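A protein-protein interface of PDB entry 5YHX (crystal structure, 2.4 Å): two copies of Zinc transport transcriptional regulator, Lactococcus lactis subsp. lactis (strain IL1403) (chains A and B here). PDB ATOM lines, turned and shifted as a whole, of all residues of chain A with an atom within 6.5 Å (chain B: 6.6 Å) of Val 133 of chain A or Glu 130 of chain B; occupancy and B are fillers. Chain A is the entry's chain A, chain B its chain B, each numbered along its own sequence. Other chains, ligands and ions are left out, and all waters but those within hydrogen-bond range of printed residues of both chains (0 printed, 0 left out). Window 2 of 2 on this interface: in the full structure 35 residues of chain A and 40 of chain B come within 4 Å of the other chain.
Val 133 of chain A touches Glu 130 of chain B, but with the chains exchanged Glu 130 of chain A does not touch Val 133 of chain B (4.1 Å).
Ile 134 of chain A touches Val 133 of chain B, but with the chains exchanged Val 133 of chain A does not touch Ile 134 of chain B (4.3 Å).
Positions printed for both chains: 128, 129, 130, 131, 132, 133, 134 and 135.
Of the 5 pairs that touch across the chains among the printed residues, none has its exchanged pair printed and touching as well.
Among the printed residues, pairs that only touch across the chains: Val 133 of chain A with Glu 130 of chain B (3.9 Å), Ile 134 of chain A with Val 133 of chain B (3.8 Å), Lys 136 of chain A with Phe 126 of chain B (3.98 Å), Phe 137 of chain A with Phe 126 of chain B (3.8 Å) and Phe 137 of chain A with Ile 134 of chain B (3.9 Å).
Of the 11 printed residues of chain A, 4 touch a printed residue of chain B.
Printed residues of chain A that touch a printed residue of chain B: Val 133, Ile 134, Lys 136 and Phe 137.
Printed residues of chain B that touch a printed residue of chain A: Phe 126, Glu 130, Val 133 and Ile 134.
Hydrophobic or aromatic side chains of chain B within 4 Å of the printed part of chain A: Phe 126, Val 133 and Ile 134.
Among the printed residues, 5 pairs touch across the chains.
Among the printed residues, no Asp or Glu carboxylate lies within 4 Å of a Lys or Arg side-chain nitrogen of the other chain.
The side-chain carboxylate (OE2) of Glu 132 of chain A lies within salt-bridge range of the side-chain amino group (NZ) of Lys 136 of chain A (3.7 Å).
The side-chain hydroxyl (OG1) of Thr 127 of chain B lies close to the side-chain carboxylate (OE1) of Glu 130 of chain B, 3.0 Å away.
The backbone carbonyl oxygen (O) of Phe 126 of chain B lies within hydrogen-bond range of the side-chain amide nitrogen (NE2) of Gln 131 of chain B.
Val 133 of chain A touches one residue of chain B.
Printed residues of chain B within 4 Å of Ile 134 of chain A: Val 133.
Of the printed residues of chain B, Lys 136 of chain A touches Phe 126 (3.98 Å).
Of the printed residues of chain B, Phe 137 of chain A touches Phe 126 and Ile 134.
Of the printed residues of chain A, Phe 126 of chain B touches Lys 136 and Phe 137.
Asp 128 of chain B touches none of the printed residues of chain A.
Of chain A, only Val 133 comes within 4 Å of Glu 130 of chain B.
The nearest printed residue of chain A that does not touch Glu 130 of chain B is Ile 134 of chain A (6.8 Å).
The nearest printed residue of chain A that does not touch Ile 134 of chain B is Val 133 of chain A (4.3 Å).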
ATOM      1  N   ASP A 128     -24.430 -28.856 -12.123  1.00  0.00           N
ATOM      2  CA  ASP A 128     -25.645 -29.644 -11.940  1.00  0.00           C
ATOM      3  C   ASP A 128     -25.806 -30.043 -10.478  1.00  0.00           C
ATOM      4  O   ASP A 128     -26.903 -29.986  -9.921  1.00  0.00           O
ATOM      5  CB  ASP A 128     -25.623 -30.907 -12.815  1.00  0.00           C
ATOM      6  CG  ASP A 128     -25.733 -30.604 -14.323  1.00  0.00           C
ATOM      7  OD1 ASP A 128     -26.366 -29.589 -14.723  1.00  0.00           O
ATOM      8  OD2 ASP A 128     -25.190 -31.410 -15.113  1.00  0.00           O
ATOM      9  N   GLU A 129     -24.701 -30.449  -9.864  1.00  0.00           N
ATOM     10  CA  GLU A 129     -24.697 -30.877  -8.475  1.00  0.00           C
ATOM     11  C   GLU A 129     -24.807 -29.687  -7.517  1.00  0.00           C
ATOM     12  O   GLU A 129     -25.389 -29.802  -6.445  1.00  0.00           O
ATOM     13  CB  GLU A 129     -23.429 -31.677  -8.181  1.00  0.00           C
ATOM     14  N   GLU A 130     -24.219 -28.555  -7.891  1.00  0.00           N
ATOM     15  CA  GLU A 130     -24.390 -27.335  -7.107  1.00  0.00           C
ATOM     16  C   GLU A 130     -25.876 -26.978  -7.074  1.00  0.00           C
ATOM     17  O   GLU A 130     -26.464 -26.780  -6.009  1.00  0.00           O
ATOM     18  CB  GLU A 130     -23.545 -26.200  -7.691  1.00  0.00           C
ATOM     19  CG  GLU A 130     -22.076 -26.267  -7.238  1.00  0.00           C
ATOM     20  CD  GLU A 130     -21.158 -25.268  -7.941  1.00  0.00           C
ATOM     21  OE1 GLU A 130     -21.360 -25.011  -9.147  1.00  0.00           O
ATOM     22  OE2 GLU A 130     -20.224 -24.740  -7.290  1.00  0.00           O
ATOM     23  N   GLN A 131     -26.478 -26.946  -8.259  1.00  0.00           N
ATOM     24  CA  GLN A 131     -27.904 -26.715  -8.409  1.00  0.00           C
ATOM     25  C   GLN A 131     -28.736 -27.622  -7.519  1.00  0.00           C
ATOM     26  O   GLN A 131     -29.750 -27.193  -6.985  1.00  0.00           O
ATOM     27  CB  GLN A 131     -28.325 -26.841  -9.876  1.00  0.00           C
ATOM     28  CG  GLN A 131     -27.637 -25.825 -10.760  1.00  0.00           C
ATOM     29  CD  GLN A 131     -28.180 -25.807 -12.178  1.00  0.00           C
ATOM     30  OE1 GLN A 131     -29.384 -25.895 -12.403  1.00  0.00           O
ATOM     31  NE2 GLN A 131     -27.288 -25.698 -13.140  1.00  0.00           N
ATOM     32  N   GLU A 132     -28.319 -28.870  -7.342  1.00  0.00           N
ATOM     33  CA  GLU A 132     -29.088 -29.770  -6.488  1.00  0.00           C
ATOM     34  C   GLU A 132     -28.911 -29.494  -4.977  1.00  0.00           C
ATOM     35  O   GLU A 132     -29.785 -29.798  -4.174  1.00  0.00           O
ATOM     36  CB  GLU A 132     -28.816 -31.240  -6.830  1.00  0.00           C
ATOM     37  CG  GLU A 132     -29.689 -32.236  -6.023  1.00  0.00           C
ATOM     38  CD  GLU A 132     -31.207 -31.924  -6.070  1.00  0.00           C
ATOM     39  OE1 GLU A 132     -31.747 -31.699  -7.189  1.00  0.00           O
ATOM     40  OE2 GLU A 132     -31.861 -31.909  -4.983  1.00  0.00           O
ATOM     41  N   VAL A 133     -27.790 -28.920  -4.576  1.00  0.00           N
ATOM     42  CA  VAL A 133     -27.675 -28.513  -3.181  1.00  0.00           C
ATOM     43  C   VAL A 133     -28.614 -27.318  -2.918  1.00  0.00           C
ATOM     44  O   VAL A 133     -29.363 -27.287  -1.942  1.00  0.00           O
ATOM     45  CB  VAL A 133     -26.236 -28.125  -2.823  1.00  0.00           C
ATOM     46  CG1 VAL A 133     -26.165 -27.698  -1.377  1.00  0.00           C
ATOM     47  CG2 VAL A 133     -25.288 -29.298  -3.095  1.00  0.00           C
ATOM     48  N   ILE A 134     -28.571 -26.348  -3.826  1.00  0.00           N
ATOM     49  CA  ILE A 134     -29.387 -25.154  -3.711  1.00  0.00           C
ATOM     50  C   ILE A 134     -30.867 -25.525  -3.710  1.00  0.00           C
ATOM     51  O   ILE A 134     -31.664 -24.888  -3.028  1.00  0.00           O
ATOM     52  CB  ILE A 134     -29.082 -24.179  -4.836  1.00  0.00           C
ATOM     53  CG1 ILE A 134     -27.605 -23.794  -4.795  1.00  0.00           C
ATOM     54  CG2 ILE A 134     -29.993 -22.951  -4.755  1.00  0.00           C
ATOM     55  CD1 ILE A 134     -27.134 -23.063  -6.069  1.00  0.00           C
ATOM     56  N   SER A 135     -31.221 -26.581  -4.439  1.00  0.00           N
ATOM     57  CA  SER A 135     -32.620 -27.022  -4.512  1.00  0.00           C
ATOM     58  C   SER A 135     -33.086 -27.603  -3.177  1.00  0.00           C
ATOM     59  O   SER A 135     -34.220 -27.393  -2.754  1.00  0.00           O
ATOM     60  CB  SER A 135     -32.818 -28.034  -5.651  1.00  0.00           C
ATOM     61  OG  SER A 135     -34.194 -28.325  -5.854  1.00  0.00           O
ATOM     62  N   LYS A 136     -32.205 -28.317  -2.496  1.00  0.00           N
ATOM     63  CA  LYS A 136     -32.537 -28.839  -1.170  1.00  0.00           C
ATOM     64  C   LYS A 136     -32.550 -27.754  -0.084  1.00  0.00           C
ATOM     65  O   LYS A 136     -33.332 -27.825   0.858  1.00  0.00           O
ATOM     66  CB  LYS A 136     -31.593 -29.984  -0.773  1.00  0.00           C
ATOM     67  CG  LYS A 136     -31.833 -31.294  -1.535  1.00  0.00           C
ATOM     68  CD  LYS A 136     -31.484 -32.510  -0.665  1.00  0.00           C
ATOM     69  CE  LYS A 136     -31.565 -33.810  -1.450  1.00  0.00           C
ATOM     70  NZ  LYS A 136     -30.358 -34.039  -2.304  1.00  0.00           N
ATOM     71  N   PHE A 137     -31.680 -26.758  -0.204  1.00  0.00           N
ATOM     72  CA  PHE A 137     -31.721 -25.628   0.729  1.00  0.00           C
ATOM     73  C   PHE A 137     -33.082 -24.921   0.673  1.00  0.00           C
ATOM     74  O   PHE A 137     -33.734 -24.717   1.698  1.00  0.00           O
ATOM     75  CB  PHE A 137     -30.602 -24.637   0.436  1.00  0.00           C
ATOM     76  CG  PHE A 137     -30.754 -23.326   1.157  1.00  0.00           C
ATOM     77  CD1 PHE A 137     -30.642 -23.263   2.539  1.00  0.00           C
ATOM     78  CD2 PHE A 137     -31.006 -22.155   0.452  1.00  0.00           C
ATOM     79  CE1 PHE A 137     -30.780 -22.072   3.202  1.00  0.00           C
ATOM     80  CE2 PHE A 137     -31.140 -20.951   1.119  1.00  0.00           C
ATOM     81  CZ  PHE A 137     -31.027 -20.911   2.499  1.00  0.00           C
ATOM     82  N   LEU A 138     -33.525 -24.600  -0.539  1.00  0.00           N
ATOM     83  CA  LEU A 138     -34.804 -23.919  -0.739  1.00  0.00           C
ATOM     84  C   LEU A 138     -36.020 -24.729  -0.271  1.00  0.00           C
ATOM     85  O   LEU A 138     -36.992 -24.142   0.223  1.00  0.00           O
ATOM     86  CB  LEU A 138     -34.973 -23.470  -2.203  1.00  0.00           C
ATOM     87  CG  LEU A 138     -34.026 -22.345  -2.663  1.00  0.00           C
ATOM     88  CD1 LEU A 138     -34.055 -22.178  -4.161  1.00  0.00           C
ATOM     89  CD2 LEU A 138     -34.408 -21.040  -2.016  1.00  0.00           C
ATOM     90  N   LYS B 125     -27.748 -28.829   8.779  1.00  0.00           N
ATOM     91  CA  LYS B 125     -28.003 -30.079   8.064  1.00  0.00           C
ATOM     92  C   LYS B 125     -27.200 -30.182   6.763  1.00  0.00           C
ATOM     93  O   LYS B 125     -27.372 -31.134   5.986  1.00  0.00           O
ATOM     94  CB  LYS B 125     -29.485 -30.220   7.725  1.00  0.00           C
ATOM     95  CG  LYS B 125     -30.382 -30.427   8.902  1.00  0.00           C
ATOM     96  CD  LYS B 125     -31.700 -31.018   8.450  1.00  0.00           C
ATOM     97  CE  LYS B 125     -32.574 -31.350   9.655  1.00  0.00           C
ATOM     98  NZ  LYS B 125     -33.918 -31.888   9.283  1.00  0.00           N
ATOM     99  N   PHE B 126     -26.339 -29.202   6.517  1.00  0.00           N
ATOM    100  CA  PHE B 126     -25.529 -29.199   5.310  1.00  0.00           C
ATOM    101  C   PHE B 126     -24.044 -29.250   5.662  1.00  0.00           C
ATOM    102  O   PHE B 126     -23.635 -28.754   6.715  1.00  0.00           O
ATOM    103  CB  PHE B 126     -25.866 -27.977   4.439  1.00  0.00           C
ATOM    104  CG  PHE B 126     -27.249 -28.028   3.848  1.00  0.00           C
ATOM    105  CD1 PHE B 126     -28.337 -27.542   4.551  1.00  0.00           C
ATOM    106  CD2 PHE B 126     -27.464 -28.581   2.592  1.00  0.00           C
ATOM    107  CE1 PHE B 126     -29.605 -27.594   4.020  1.00  0.00           C
ATOM    108  CE2 PHE B 126     -28.741 -28.641   2.056  1.00  0.00           C
ATOM    109  CZ  PHE B 126     -29.815 -28.144   2.778  1.00  0.00           C
ATOM    110  N   THR B 127     -23.244 -29.866   4.793  1.00  0.00           N
ATOM    111  CA  THR B 127     -21.807 -29.959   5.027  1.00  0.00           C
ATOM    112  C   THR B 127     -21.152 -28.598   4.865  1.00  0.00           C
ATOM    113  O   THR B 127     -21.751 -27.675   4.313  1.00  0.00           O
ATOM    114  CB  THR B 127     -21.114 -30.977   4.084  1.00  0.00           C
ATOM    115  OG1 THR B 127     -21.244 -30.551   2.722  1.00  0.00           O
ATOM    116  CG2 THR B 127     -21.729 -32.364   4.239  1.00  0.00           C
ATOM    117  N   ASP B 128     -19.923 -28.485   5.353  1.00  0.00           N
ATOM    118  CA  ASP B 128     -19.166 -27.242   5.283  1.00  0.00           C
ATOM    119  C   ASP B 128     -19.151 -26.651   3.861  1.00  0.00           C
ATOM    120  O   ASP B 128     -19.457 -25.473   3.675  1.00  0.00           O
ATOM    121  CB  ASP B 128     -17.736 -27.471   5.811  1.00  0.00           C
ATOM    122  CG  ASP B 128     -16.982 -26.165   6.115  1.00  0.00           C
ATOM    123  OD1 ASP B 128     -17.630 -25.094   6.228  1.00  0.00           O
ATOM    124  OD2 ASP B 128     -15.735 -26.221   6.259  1.00  0.00           O
ATOM    125  N   GLU B 129     -18.814 -27.461   2.859  1.00  0.00           N
ATOM    126  CA  GLU B 129     -18.588 -26.917   1.512  1.00  0.00           C
ATOM    127  C   GLU B 129     -19.873 -26.701   0.723  1.00  0.00           C
ATOM    128  O   GLU B 129     -19.887 -25.934  -0.244  1.00  0.00           O
ATOM    129  CB  GLU B 129     -17.606 -27.774   0.702  1.00  0.00           C
ATOM    130  CG  GLU B 129     -18.151 -29.124   0.235  1.00  0.00           C
ATOM    131  CD  GLU B 129     -17.121 -29.935  -0.549  1.00  0.00           C
ATOM    132  OE1 GLU B 129     -16.651 -29.459  -1.611  1.00  0.00           O
ATOM    133  OE2 GLU B 129     -16.777 -31.048  -0.088  1.00  0.00           O
ATOM    134  N   GLU B 130     -20.934 -27.396   1.136  1.00  0.00           N
ATOM    135  CA  GLU B 130     -22.280 -27.178   0.615  1.00  0.00           C
ATOM    136  C   GLU B 130     -22.812 -25.841   1.149  1.00  0.00           C
ATOM    137  O   GLU B 130     -23.411 -25.046   0.408  1.00  0.00           O
ATOM    138  CB  GLU B 130     -23.201 -28.324   1.032  1.00  0.00           C
ATOM    139  CG  GLU B 130     -22.830 -29.685   0.433  1.00  0.00           C
ATOM    140  CD  GLU B 130     -23.719 -30.832   0.938  1.00  0.00           C
ATOM    141  OE1 GLU B 130     -24.129 -30.815   2.124  1.00  0.00           O
ATOM    142  OE2 GLU B 130     -24.011 -31.753   0.140  1.00  0.00           O
ATOM    143  N   GLN B 131     -22.568 -25.602   2.437  1.00  0.00           N
ATOM    144  CA  GLN B 131     -22.887 -24.336   3.082  1.00  0.00           C
ATOM    145  C   GLN B 131     -22.272 -23.161   2.338  1.00  0.00           C
ATOM    146  O   GLN B 131     -22.865 -22.086   2.276  1.00  0.00           O
ATOM    147  CB  GLN B 131     -22.409 -24.328   4.530  1.00  0.00           C
ATOM    148  CG  GLN B 131     -23.284 -25.152   5.469  1.00  0.00           C
ATOM    149  CD  GLN B 131     -23.075 -24.810   6.938  1.00  0.00           C
ATOM    150  OE1 GLN B 131     -22.618 -23.717   7.278  1.00  0.00           O
ATOM    151  NE2 GLN B 131     -23.405 -25.751   7.813  1.00  0.00           N
ATOM    152  N   GLU B 132     -21.084 -23.358   1.777  1.00  0.00           N
ATOM    153  CA  GLU B 132     -20.458 -22.289   1.013  1.00  0.00           C
ATOM    154  C   GLU B 132     -21.139 -22.146  -0.355  1.00  0.00           C
ATOM    155  O   GLU B 132     -21.133 -21.063  -0.956  1.00  0.00           O
ATOM    156  CB  GLU B 132     -18.951 -22.525   0.860  1.00  0.00           C
ATOM    157  CG  GLU B 132     -18.187 -21.317   0.315  1.00  0.00           C
ATOM    158  CD  GLU B 132     -18.354 -20.060   1.182  1.00  0.00           C
ATOM    159  OE1 GLU B 132     -18.382 -20.191   2.433  1.00  0.00           O
ATOM    160  OE2 GLU B 132     -18.466 -18.944   0.607  1.00  0.00           O
ATOM    161  N   VAL B 133     -21.733 -23.235  -0.843  1.00  0.00           N
ATOM    162  CA  VAL B 133     -22.504 -23.181  -2.089  1.00  0.00           C
ATOM    163  C   VAL B 133     -23.721 -22.284  -1.917  1.00  0.00           C
ATOM    164  O   VAL B 133     -23.993 -21.402  -2.735  1.00  0.00           O
ATOM    165  CB  VAL B 133     -23.008 -24.573  -2.536  1.00  0.00           C
ATOM    166  CG1 VAL B 133     -24.071 -24.424  -3.634  1.00  0.00           C
ATOM    167  CG2 VAL B 133     -21.848 -25.442  -3.004  1.00  0.00           C
ATOM    168  N   ILE B 134     -24.445 -22.541  -0.839  1.00  0.00           N
ATOM    169  CA  ILE B 134     -25.624 -21.781  -0.494  1.00  0.00           C
ATOM    170  C   ILE B 134     -25.288 -20.306  -0.357  1.00  0.00           C
ATOM    171  O   ILE B 134     -25.846 -19.458  -1.067  1.00  0.00           O
ATOM    172  CB  ILE B 134     -26.240 -22.321   0.799  1.00  0.00           C
ATOM    173  CG1 ILE B 134     -26.848 -23.701   0.520  1.00  0.00           C
ATOM    174  CG2 ILE B 134     -27.283 -21.368   1.331  1.00  0.00           C
ATOM    175  CD1 ILE B 134     -26.736 -24.677   1.658  1.00  0.00           C
ATOM    176  N   SER B 135     -24.363 -20.003   0.537  1.00  0.00           N
ATOM    177  CA  SER B 135     -23.919 -18.627   0.706  1.00  0.00           C
ATOM    178  C   SER B 135     -23.668 -17.978  -0.647  1.00  0.00           C
ATOM    179  O   SER B 135     -24.125 -16.858  -0.914  1.00  0.00           O
ATOM    180  CB  SER B 135     -22.641 -18.581   1.531  1.00  0.00           C
ATOM    181  OG  SER B 135     -22.125 -17.267   1.546  1.00  0.00           O
